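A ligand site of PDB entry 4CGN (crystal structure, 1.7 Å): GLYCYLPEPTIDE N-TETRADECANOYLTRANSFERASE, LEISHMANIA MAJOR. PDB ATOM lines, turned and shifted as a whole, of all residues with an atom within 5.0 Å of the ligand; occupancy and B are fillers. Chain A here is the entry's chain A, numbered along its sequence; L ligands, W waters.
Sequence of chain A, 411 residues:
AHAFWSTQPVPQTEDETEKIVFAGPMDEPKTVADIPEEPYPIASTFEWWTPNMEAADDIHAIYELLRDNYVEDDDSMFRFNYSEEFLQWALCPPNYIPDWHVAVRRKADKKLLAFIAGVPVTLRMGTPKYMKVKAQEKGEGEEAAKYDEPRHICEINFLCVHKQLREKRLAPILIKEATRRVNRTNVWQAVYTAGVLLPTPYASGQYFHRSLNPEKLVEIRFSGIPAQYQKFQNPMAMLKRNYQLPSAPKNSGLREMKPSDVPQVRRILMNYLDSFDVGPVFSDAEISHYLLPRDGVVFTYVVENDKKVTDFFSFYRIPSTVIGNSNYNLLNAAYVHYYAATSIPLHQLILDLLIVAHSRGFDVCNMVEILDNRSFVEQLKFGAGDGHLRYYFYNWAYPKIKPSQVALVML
The side-chain amide nitrogen (ND2) of Asn 366 is in hydrogen-bond range of an oxygen (O1) of the ligand, at 3.2 Å. N3 of the ligand lies within salt-bridge range of O of Leu 411 (2.8 Å). OH of Tyr 335 is in hydrogen-bond range of O1 of the ligand, at 2.7 Å.
N of Tyr 335 sits at hydrogen-bond distance from O of Tyr 316 (2.9 Å). ND1 of His 209 lies within hydrogen-bond range of OD1 of Asn 366, 2.6 Å away. The backbone carbonyl oxygen (O) of Ser 320 lies within hydrogen-bond range of the backbone NH (N) of Leu 331, at 2.8 Å. The backbone carbonyl oxygen (O) of Val 71 is in hydrogen-bond range of the backbone NH (N) of Phe 80, at 3.0 Å. OH of Tyr 335 is in hydrogen-bond range of ND2 of Asn 366. The side-chain hydroxyl (OH) of Tyr 316 lies within hydrogen-bond range of the backbone carbonyl oxygen (O) of Met 410, at 3.2 Å. OE2 of Glu 72 is in salt-bridge range of NH1 of Arg 79 (2.9 Å). The chain-end carboxylate (O) of Leu 411 lies within hydrogen-bond range of the side-chain amide nitrogen (ND2) of Asn 157, at 2.9 Å.
Water W6 lies within hydrogen-bond range of the side-chain hydroxyl of Tyr 70 (2.7 Å), the side-chain amide oxygen of Asn 157 (2.8 Å), the side-chain hydroxyl of Tyr 82 (2.8 Å), a nitrogen (N3) of the ligand (2.8 Å) and the chain-end carboxylate of Leu 411 (3.2 Å). Water W7 lies within hydrogen-bond range of ND2 of Asn 366, O1 of the ligand and OH of Tyr 335. Water W5 bridges the side-chain hydroxyl (OH) of Tyr 70 and a nitrogen (N3) of the ligand. Water W3 lies within hydrogen-bond range of the side-chain hydroxyl (OH) of Tyr 316 (2.7 Å), the chain-end carboxylate (OXT) of Leu 411 (2.9 Å) and the backbone carbonyl oxygen (O) of Met 410 (3.4 Å). Water W2 bridges O of Thr 193 (2.8 Å) and OD1 of Asn 157 (3.4 Å).
The backbone carbonyl oxygen of Val 71 lies close to a fluorine (F1) of the ligand (3.4 Å). F1 of the ligand lies close to O of Phe 78 (3.3 Å). The backbone NH (N) of Phe 80 lies close to a fluorine (F1) of the ligand (3.3 Å). Residues that only touch the ligand: Ser 320 (3.1 Å), Tyr 82 (3.3 Å), Arg 79 (3.4 Å), Tyr 207 (3.5 Å), Asp 73 (3.5 Å), Thr 193 (3.6 Å), Val 368 (3.6 Å), Met 410 (3.6 Å), Glu 72 (3.7 Å), Met 367 (3.8 Å) and Leu 389 (3.9 Å). Hydrophobic or aromatic side chains within 4 Å of the ligand: Phe 78, Phe 80, Tyr 207, Tyr 335, Val 368 and Leu 389. Within 4 Å of the ligand: Val 71, Glu 72, Asp 73, Phe 78, Arg 79, Phe 80, Tyr 82, Thr 193, Tyr 207, Ser 320, Tyr 335, Asn 366, Met 367, Val 368, Leu 389, Met 410 and Leu 411. The nearest printed residue that does not touch the ligand is His 209 (4.1 Å).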
ATOM      1  N   TYR A  70      -7.754  -0.833  31.097  1.00  0.00           N
ATOM      2  CA  TYR A  70      -7.576   0.597  30.828  1.00  0.00           C
ATOM      3  C   TYR A  70      -7.371   0.928  29.327  1.00  0.00           C
ATOM      4  O   TYR A  70      -7.730   0.124  28.459  1.00  0.00           O
ATOM      5  CB  TYR A  70      -6.437   1.136  31.730  1.00  0.00           C
ATOM      6  CG  TYR A  70      -6.391   2.661  31.933  1.00  0.00           C
ATOM      7  CD1 TYR A  70      -7.561   3.376  32.255  1.00  0.00           C
ATOM      8  CD2 TYR A  70      -5.160   3.377  31.807  1.00  0.00           C
ATOM      9  CE1 TYR A  70      -7.516   4.774  32.426  1.00  0.00           C
ATOM     10  CE2 TYR A  70      -5.099   4.775  32.006  1.00  0.00           C
ATOM     11  CZ  TYR A  70      -6.285   5.456  32.289  1.00  0.00           C
ATOM     12  OH  TYR A  70      -6.301   6.817  32.490  1.00  0.00           O
ATOM     13  N   VAL A  71      -6.768   2.094  29.034  1.00  0.00           N
ATOM     14  CA  VAL A  71      -6.754   2.615  27.676  1.00  0.00           C
ATOM     15  C   VAL A  71      -5.915   1.698  26.703  1.00  0.00           C
ATOM     16  O   VAL A  71      -4.846   1.268  27.056  1.00  0.00           O
ATOM     17  CB  VAL A  71      -6.058   3.991  27.707  1.00  0.00           C
ATOM     18  CG1 VAL A  71      -5.932   4.540  26.321  1.00  0.00           C
ATOM     19  CG2 VAL A  71      -6.933   5.010  28.543  1.00  0.00           C
ATOM     20  N   GLU A  72      -6.470   1.373  25.554  1.00  0.00           N
ATOM     21  CA  GLU A  72      -5.700   0.694  24.502  1.00  0.00           C
ATOM     22  C   GLU A  72      -5.476   1.634  23.311  1.00  0.00           C
ATOM     23  O   GLU A  72      -6.119   2.673  23.206  1.00  0.00           O
ATOM     24  CB  GLU A  72      -6.503  -0.511  24.013  1.00  0.00           C
ATOM     25  CG  GLU A  72      -6.766  -1.485  25.156  1.00  0.00           C
ATOM     26  CD  GLU A  72      -7.768  -2.612  24.847  1.00  0.00           C
ATOM     27  OE1 GLU A  72      -8.263  -2.752  23.705  1.00  0.00           O
ATOM     28  OE2 GLU A  72      -8.043  -3.389  25.782  1.00  0.00           O
ATOM     29  N   ASP A  73      -4.601   1.232  22.407  1.00  0.00           N
ATOM     30  CA  ASP A  73      -4.504   1.911  21.122  1.00  0.00           C
ATOM     31  C   ASP A  73      -5.762   1.524  20.303  1.00  0.00           C
ATOM     32  O   ASP A  73      -6.635   0.778  20.745  1.00  0.00           O
ATOM     33  CB  ASP A  73      -3.261   1.402  20.379  1.00  0.00           C
ATOM     34  CG  ASP A  73      -3.443  -0.015  19.894  1.00  0.00           C
ATOM     35  OD1 ASP A  73      -3.679  -0.928  20.735  1.00  0.00           O
ATOM     36  OD2 ASP A  73      -3.360  -0.253  18.646  1.00  0.00           O
ATOM     37  N   PHE A  78      -2.109  -2.646  21.857  1.00  0.00           N
ATOM     38  CA  PHE A  78      -1.416  -2.261  23.054  1.00  0.00           C
ATOM     39  C   PHE A  78      -2.393  -1.805  24.106  1.00  0.00           C
ATOM     40  O   PHE A  78      -3.434  -1.237  23.770  1.00  0.00           O
ATOM     41  CB  PHE A  78      -0.543  -1.022  22.739  1.00  0.00           C
ATOM     42  CG  PHE A  78       0.394  -1.252  21.574  1.00  0.00           C
ATOM     43  CD1 PHE A  78       1.428  -2.190  21.694  1.00  0.00           C
ATOM     44  CD2 PHE A  78       0.094  -0.695  20.319  1.00  0.00           C
ATOM     45  CE1 PHE A  78       2.244  -2.461  20.600  1.00  0.00           C
ATOM     46  CE2 PHE A  78       0.919  -0.951  19.210  1.00  0.00           C
ATOM     47  CZ  PHE A  78       1.940  -1.859  19.369  1.00  0.00           C
ATOM     48  N   ARG A  79      -2.040  -2.002  25.353  1.00  0.00           N
ATOM     49  CA  ARG A  79      -2.886  -1.424  26.440  1.00  0.00           C
ATOM     50  C   ARG A  79      -1.909  -0.901  27.525  1.00  0.00           C
ATOM     51  O   ARG A  79      -0.918  -1.574  27.947  1.00  0.00           O
ATOM     52  CB  ARG A  79      -3.819  -2.529  27.040  1.00  0.00           C
ATOM     53  CG  ARG A  79      -4.737  -2.011  28.209  1.00  0.00           C
ATOM     54  CD  ARG A  79      -5.914  -3.014  28.439  1.00  0.00           C
ATOM     55  NE  ARG A  79      -5.402  -4.360  28.681  1.00  0.00           N
ATOM     56  CZ  ARG A  79      -5.594  -5.443  27.912  1.00  0.00           C
ATOM     57  NH1 ARG A  79      -6.283  -5.442  26.767  1.00  0.00           N
ATOM     58  NH2 ARG A  79      -5.014  -6.583  28.315  1.00  0.00           N
ATOM     59  N   PHE A  80      -2.167   0.309  28.067  1.00  0.00           N
ATOM     60  CA  PHE A  80      -1.206   0.812  29.032  1.00  0.00           C
ATOM     61  C   PHE A  80      -1.077  -0.113  30.216  1.00  0.00           C
ATOM     62  O   PHE A  80      -2.090  -0.731  30.616  1.00  0.00           O
ATOM     63  CB  PHE A  80      -1.714   2.149  29.586  1.00  0.00           C
ATOM     64  CG  PHE A  80      -1.538   3.280  28.655  1.00  0.00           C
ATOM     65  CD1 PHE A  80      -0.332   3.644  28.246  1.00  0.00           C
ATOM     66  CD2 PHE A  80      -2.642   4.057  28.263  1.00  0.00           C
ATOM     67  CE1 PHE A  80      -0.176   4.770  27.364  1.00  0.00           C
ATOM     68  CE2 PHE A  80      -2.493   5.182  27.402  1.00  0.00           C
ATOM     69  CZ  PHE A  80      -1.246   5.493  26.929  1.00  0.00           C
ATOM     70  N   TYR A  82       0.474   0.807  33.552  1.00  0.00           N
ATOM     71  CA  TYR A  82       1.106   1.572  34.600  1.00  0.00           C
ATOM     72  C   TYR A  82       1.540   0.666  35.733  1.00  0.00           C
ATOM     73  O   TYR A  82       0.775  -0.208  36.160  1.00  0.00           O
ATOM     74  CB  TYR A  82       0.025   2.551  35.136  1.00  0.00           C
ATOM     75  CG  TYR A  82      -0.283   3.725  34.183  1.00  0.00           C
ATOM     76  CD1 TYR A  82      -1.313   3.624  33.223  1.00  0.00           C
ATOM     77  CD2 TYR A  82       0.420   4.958  34.312  1.00  0.00           C
ATOM     78  CE1 TYR A  82      -1.608   4.694  32.399  1.00  0.00           C
ATOM     79  CE2 TYR A  82       0.094   6.063  33.541  1.00  0.00           C
ATOM     80  CZ  TYR A  82      -0.877   5.925  32.593  1.00  0.00           C
ATOM     81  OH  TYR A  82      -1.191   7.034  31.808  1.00  0.00           O
ATOM     82  N   ASN A 157      -7.785  11.553  36.823  1.00  0.00           N
ATOM     83  CA  ASN A 157      -7.104  10.606  35.863  1.00  0.00           C
ATOM     84  C   ASN A 157      -7.568   9.205  36.258  1.00  0.00           C
ATOM     85  O   ASN A 157      -8.265   9.014  37.287  1.00  0.00           O
ATOM     86  CB  ASN A 157      -5.562  10.815  35.973  1.00  0.00           C
ATOM     87  CG  ASN A 157      -4.801  10.455  34.687  1.00  0.00           C
ATOM     88  OD1 ASN A 157      -5.270   9.735  33.858  1.00  0.00           O
ATOM     89  ND2 ASN A 157      -3.558  10.904  34.620  1.00  0.00           N
ATOM     90  N   THR A 193      -7.673  15.156  31.053  1.00  0.00           N
ATOM     91  CA  THR A 193      -7.471  15.023  29.614  1.00  0.00           C
ATOM     92  C   THR A 193      -8.156  13.721  29.143  1.00  0.00           C
ATOM     93  O   THR A 193      -8.504  12.828  29.944  1.00  0.00           O
ATOM     94  CB  THR A 193      -5.984  14.969  29.234  1.00  0.00           C
ATOM     95  OG1 THR A 193      -5.347  13.884  29.932  1.00  0.00           O
ATOM     96  CG2 THR A 193      -5.228  16.247  29.567  1.00  0.00           C
ATOM     97  N   TYR A 207      -0.137  13.759  19.464  1.00  0.00           N
ATOM     98  CA  TYR A 207       0.944  13.003  20.066  1.00  0.00           C
ATOM     99  C   TYR A 207       2.115  12.932  19.141  1.00  0.00           C
ATOM    100  O   TYR A 207       1.910  12.968  17.904  1.00  0.00           O
ATOM    101  CB  TYR A 207       0.461  11.587  20.284  1.00  0.00           C
ATOM    102  CG  TYR A 207      -0.829  11.446  21.111  1.00  0.00           C
ATOM    103  CD1 TYR A 207      -0.816  11.553  22.487  1.00  0.00           C
ATOM    104  CD2 TYR A 207      -2.026  11.086  20.497  1.00  0.00           C
ATOM    105  CE1 TYR A 207      -1.962  11.321  23.261  1.00  0.00           C
ATOM    106  CE2 TYR A 207      -3.192  10.865  21.256  1.00  0.00           C
ATOM    107  CZ  TYR A 207      -3.145  10.967  22.633  1.00  0.00           C
ATOM    108  OH  TYR A 207      -4.303  10.762  23.419  1.00  0.00           O
ATOM    109  N   HIS A 209       6.001  10.725  18.648  1.00  0.00           N
ATOM    110  CA  HIS A 209       6.851   9.547  19.047  1.00  0.00           C
ATOM    111  C   HIS A 209       8.223   9.674  18.471  1.00  0.00           C
ATOM    112  O   HIS A 209       8.363  10.073  17.297  1.00  0.00           O
ATOM    113  CB  HIS A 209       6.255   8.269  18.498  1.00  0.00           C
ATOM    114  CG  HIS A 209       4.805   8.146  18.823  1.00  0.00           C
ATOM    115  ND1 HIS A 209       4.337   8.125  20.120  1.00  0.00           N
ATOM    116  CD2 HIS A 209       3.722   8.035  18.019  1.00  0.00           C
ATOM    117  CE1 HIS A 209       3.023   8.035  20.105  1.00  0.00           C
ATOM    118  NE2 HIS A 209       2.620   8.007  18.848  1.00  0.00           N
ATOM    119  N   PHE A 222       4.065  -1.174  16.335  1.00  0.00           N
ATOM    120  CA  PHE A 222       3.943   0.205  16.780  1.00  0.00           C
ATOM    121  C   PHE A 222       4.256   1.158  15.633  1.00  0.00           C
ATOM    122  O   PHE A 222       3.568   2.124  15.462  1.00  0.00           O
ATOM    123  CB  PHE A 222       4.883   0.451  17.959  1.00  0.00           C
ATOM    124  CG  PHE A 222       4.808   1.850  18.496  1.00  0.00           C
ATOM    125  CD1 PHE A 222       5.557   2.882  17.941  1.00  0.00           C
ATOM    126  CD2 PHE A 222       4.036   2.112  19.627  1.00  0.00           C
ATOM    127  CE1 PHE A 222       5.501   4.177  18.459  1.00  0.00           C
ATOM    128  CE2 PHE A 222       3.997   3.405  20.160  1.00  0.00           C
ATOM    129  CZ  PHE A 222       4.723   4.434  19.569  1.00  0.00           C
ATOM    130  N   TYR A 316       9.030  10.200  32.373  1.00  0.00           N
ATOM    131  CA  TYR A 316       8.555   9.083  33.219  1.00  0.00           C
ATOM    132  C   TYR A 316       8.243   7.856  32.360  1.00  0.00           C
ATOM    133  O   TYR A 316       8.173   7.936  31.137  1.00  0.00           O
ATOM    134  CB  TYR A 316       7.327   9.565  34.065  1.00  0.00           C
ATOM    135  CG  TYR A 316       6.224  10.176  33.226  1.00  0.00           C
ATOM    136  CD1 TYR A 316       5.213   9.416  32.616  1.00  0.00           C
ATOM    137  CD2 TYR A 316       6.185  11.552  33.007  1.00  0.00           C
ATOM    138  CE1 TYR A 316       4.194   9.987  31.868  1.00  0.00           C
ATOM    139  CE2 TYR A 316       5.214  12.121  32.232  1.00  0.00           C
ATOM    140  CZ  TYR A 316       4.214  11.372  31.678  1.00  0.00           C
ATOM    141  OH  TYR A 316       3.314  12.022  30.912  1.00  0.00           O
ATOM    142  N   ILE A 318       5.956   4.654  31.215  1.00  0.00           N
ATOM    143  CA  ILE A 318       4.730   3.876  31.254  1.00  0.00           C
ATOM    144  C   ILE A 318       4.955   2.782  30.246  1.00  0.00           C
ATOM    145  O   ILE A 318       4.950   3.041  29.045  1.00  0.00           O
ATOM    146  CB  ILE A 318       3.445   4.625  30.896  1.00  0.00           C
ATOM    147  CG1 ILE A 318       3.293   5.964  31.664  1.00  0.00           C
ATOM    148  CG2 ILE A 318       2.282   3.696  31.248  1.00  0.00           C
ATOM    149  CD1 ILE A 318       2.295   6.918  30.955  1.00  0.00           C
ATOM    150  N   SER A 320       3.579  -0.524  28.095  1.00  0.00           N
ATOM    151  CA  SER A 320       2.295  -1.009  27.539  1.00  0.00           C
ATOM    152  C   SER A 320       2.390  -2.471  27.292  1.00  0.00           C
ATOM    153  O   SER A 320       3.438  -2.985  26.885  1.00  0.00           O
ATOM    154  CB  SER A 320       1.916  -0.305  26.234  1.00  0.00           C
ATOM    155  OG  SER A 320       1.444   0.984  26.594  1.00  0.00           O
ATOM    156  N   LEU A 331       5.959  -2.971  25.629  1.00  0.00           N
ATOM    157  CA  LEU A 331       6.584  -1.782  25.015  1.00  0.00           C
ATOM    158  C   LEU A 331       7.074  -0.833  26.137  1.00  0.00           C
ATOM    159  O   LEU A 331       6.291  -0.507  27.070  1.00  0.00           O
ATOM    160  CB  LEU A 331       5.534  -1.083  24.241  1.00  0.00           C
ATOM    161  CG  LEU A 331       5.891   0.378  23.853  1.00  0.00           C
ATOM    162  CD1 LEU A 331       6.902   0.322  22.731  1.00  0.00           C
ATOM    163  CD2 LEU A 331       4.656   1.114  23.342  1.00  0.00           C
ATOM    164  N   TYR A 335       8.117   9.109  28.471  1.00  0.00           N
ATOM    165  CA  TYR A 335       7.236  10.259  28.174  1.00  0.00           C
ATOM    166  C   TYR A 335       7.933  11.503  28.664  1.00  0.00           C
ATOM    167  O   TYR A 335       8.347  11.617  29.835  1.00  0.00           O
ATOM    168  CB  TYR A 335       5.931  10.065  28.984  1.00  0.00           C
ATOM    169  CG  TYR A 335       5.122   8.967  28.372  1.00  0.00           C
ATOM    170  CD1 TYR A 335       5.384   7.620  28.693  1.00  0.00           C
ATOM    171  CD2 TYR A 335       4.084   9.232  27.544  1.00  0.00           C
ATOM    172  CE1 TYR A 335       4.678   6.616  28.069  1.00  0.00           C
ATOM    173  CE2 TYR A 335       3.304   8.204  26.926  1.00  0.00           C
ATOM    174  CZ  TYR A 335       3.651   6.876  27.248  1.00  0.00           C
ATOM    175  OH  TYR A 335       2.972   5.816  26.615  1.00  0.00           O
ATOM    176  N   ASN A 366       7.838   9.481  23.974  1.00  0.00           N
ATOM    177  CA  ASN A 366       6.547  10.042  23.548  1.00  0.00           C
ATOM    178  C   ASN A 366       6.328  11.404  24.191  1.00  0.00           C
ATOM    179  O   ASN A 366       6.841  11.700  25.249  1.00  0.00           O
ATOM    180  CB  ASN A 366       5.414   9.122  24.070  1.00  0.00           C
ATOM    181  CG  ASN A 366       5.463   7.759  23.465  1.00  0.00           C
ATOM    182  OD1 ASN A 366       5.742   7.621  22.262  1.00  0.00           O
ATOM    183  ND2 ASN A 366       5.128   6.709  24.294  1.00  0.00           N
ATOM    184  N   MET A 367       5.498  12.222  23.547  1.00  0.00           N
ATOM    185  CA  MET A 367       5.105  13.517  24.136  1.00  0.00           C
ATOM    186  C   MET A 367       3.878  14.032  23.388  1.00  0.00           C
ATOM    187  O   MET A 367       3.466  13.479  22.390  1.00  0.00           O
ATOM    188  CB  MET A 367       6.225  14.562  24.050  1.00  0.00           C
ATOM    189  CG  MET A 367       6.506  14.934  22.590  1.00  0.00           C
ATOM    190  SD  MET A 367       7.949  15.995  22.552  1.00  0.00           S
ATOM    191  CE  MET A 367       8.034  16.353  20.770  1.00  0.00           C
ATOM    192  N   VAL A 368       3.275  15.077  23.937  1.00  0.00           N
ATOM    193  CA  VAL A 368       2.189  15.805  23.181  1.00  0.00           C
ATOM    194  C   VAL A 368       2.818  17.160  22.865  1.00  0.00           C
ATOM    195  O   VAL A 368       3.770  17.573  23.526  1.00  0.00           O
ATOM    196  CB  VAL A 368       0.981  15.970  24.104  1.00  0.00           C
ATOM    197  CG1 VAL A 368      -0.150  16.812  23.487  1.00  0.00           C
ATOM    198  CG2 VAL A 368       0.408  14.596  24.409  1.00  0.00           C
ATOM    199  N   LEU A 389      -4.559  14.422  22.094  1.00  0.00           N
ATOM    200  CA  LEU A 389      -4.897  14.477  23.523  1.00  0.00           C
ATOM    201  C   LEU A 389      -5.662  15.796  23.682  1.00  0.00           C
ATOM    202  O   LEU A 389      -5.145  16.841  23.269  1.00  0.00           O
ATOM    203  CB  LEU A 389      -3.588  14.547  24.378  1.00  0.00           C
ATOM    204  CG  LEU A 389      -3.959  14.413  25.865  1.00  0.00           C
ATOM    205  CD1 LEU A 389      -4.617  13.073  26.242  1.00  0.00           C
ATOM    206  CD2 LEU A 389      -2.745  14.550  26.740  1.00  0.00           C
ATOM    207  N   MET A 410       0.196  15.708  31.677  1.00  0.00           N
ATOM    208  CA  MET A 410      -0.765  14.829  32.342  1.00  0.00           C
ATOM    209  C   MET A 410      -0.251  13.412  32.185  1.00  0.00           C
ATOM    210  O   MET A 410       0.250  13.015  31.124  1.00  0.00           O
ATOM    211  CB  MET A 410      -2.213  15.063  31.855  1.00  0.00           C
ATOM    212  CG  MET A 410      -2.755  16.449  32.283  1.00  0.00           C
ATOM    213  SD  MET A 410      -3.485  16.545  33.912  1.00  0.00           S
ATOM    214  CE  MET A 410      -5.123  15.892  33.618  1.00  0.00           C
ATOM    215  N   LEU A 411      -0.374  12.667  33.269  1.00  0.00           N
ATOM    216  CA  LEU A 411       0.228  11.337  33.335  1.00  0.00           C
ATOM    217  C   LEU A 411      -0.613  10.267  32.592  1.00  0.00           C
ATOM    218  O   LEU A 411      -1.818  10.398  32.361  1.00  0.00           O
ATOM    219  CB  LEU A 411       0.533  10.971  34.815  1.00  0.00           C
ATOM    220  CG  LEU A 411       1.478  11.925  35.570  1.00  0.00           C
ATOM    221  CD1 LEU A 411       1.564  11.509  37.043  1.00  0.00           C
ATOM    222  CD2 LEU A 411       2.855  12.040  34.953  1.00  0.00           C
ATOM    223  OXT LEU A 411      -0.028   9.214  32.164  1.00  0.00           O
HETATM  224  O1  LIG L   1       1.934   6.246  24.168  1.00  0.00           O
HETATM  225  C1  LIG L   1       1.028   6.565  23.353  1.00  0.00           C
HETATM  226  C2  LIG L   1       0.632   5.553  22.267  1.00  0.00           C
HETATM  227  C3  LIG L   1      -0.037   4.443  22.994  1.00  0.00           C
HETATM  228  C4  LIG L   1       0.681   3.431  23.581  1.00  0.00           C
HETATM  229  C5  LIG L   1      -0.062   2.441  24.310  1.00  0.00           C
HETATM  230  C6  LIG L   1      -1.452   4.431  23.026  1.00  0.00           C
HETATM  231  C7  LIG L   1      -2.186   3.440  23.706  1.00  0.00           C
HETATM  232  C8  LIG L   1      -1.447   2.468  24.354  1.00  0.00           C
HETATM  233  F1  LIG L   1      -2.168   1.512  24.988  1.00  0.00           F
HETATM  234  N1  LIG L   1       0.379   7.797  23.309  1.00  0.00           N
HETATM  235  C9  LIG L   1       0.665   8.867  24.174  1.00  0.00           C
HETATM  236  C10 LIG L   1      -0.145   9.175  25.286  1.00  0.00           C
HETATM  237  C11 LIG L   1       0.173  10.259  26.129  1.00  0.00           C
HETATM  238  C12 LIG L   1       1.304  11.077  25.836  1.00  0.00           C
HETATM  239  C13 LIG L   1       2.084  10.799  24.721  1.00  0.00           C
HETATM  240  C14 LIG L   1       1.801   9.676  23.881  1.00  0.00           C
HETATM  241  C15 LIG L   1      -0.405  10.851  27.285  1.00  0.00           C
HETATM  242  C16 LIG L   1       0.329  11.936  27.684  1.00  0.00           C
HETATM  243  N2  LIG L   1       1.397  12.095  26.772  1.00  0.00           N
HETATM  244  C17 LIG L   1      -1.654  10.358  27.959  1.00  0.00           C
HETATM  245  C18 LIG L   1      -1.379   9.000  28.680  1.00  0.00           C
HETATM  246  C19 LIG L   1      -2.721   8.482  29.205  1.00  0.00           C
HETATM  247  N3  LIG L   1      -3.267   9.506  30.176  1.00  0.00           N
HETATM  248  C20 LIG L   1      -3.566  10.807  29.566  1.00  0.00           C
HETATM  249  C21 LIG L   1      -2.258  11.360  28.994  1.00  0.00           C
HETATM  250  O   HOH W   1      -3.160   7.042  24.066  1.00  0.00           O
HETATM  251  O   HOH W   2      -6.617  11.239  31.162  1.00  0.00           O
HETATM  252  O   HOH W   3       1.584  10.135  29.971  1.00  0.00           O
HETATM  253  O   HOH W   4      -1.781   8.043  21.576  1.00  0.00           O
HETATM  254  O   HOH W   5      -6.030   8.684  30.403  1.00  0.00           O
HETATM  255  O   HOH W   6      -3.811   7.871  32.442  1.00  0.00           O
HETATM  256  O   HOH W   7       3.925   4.159  23.998  1.00  0.00           O
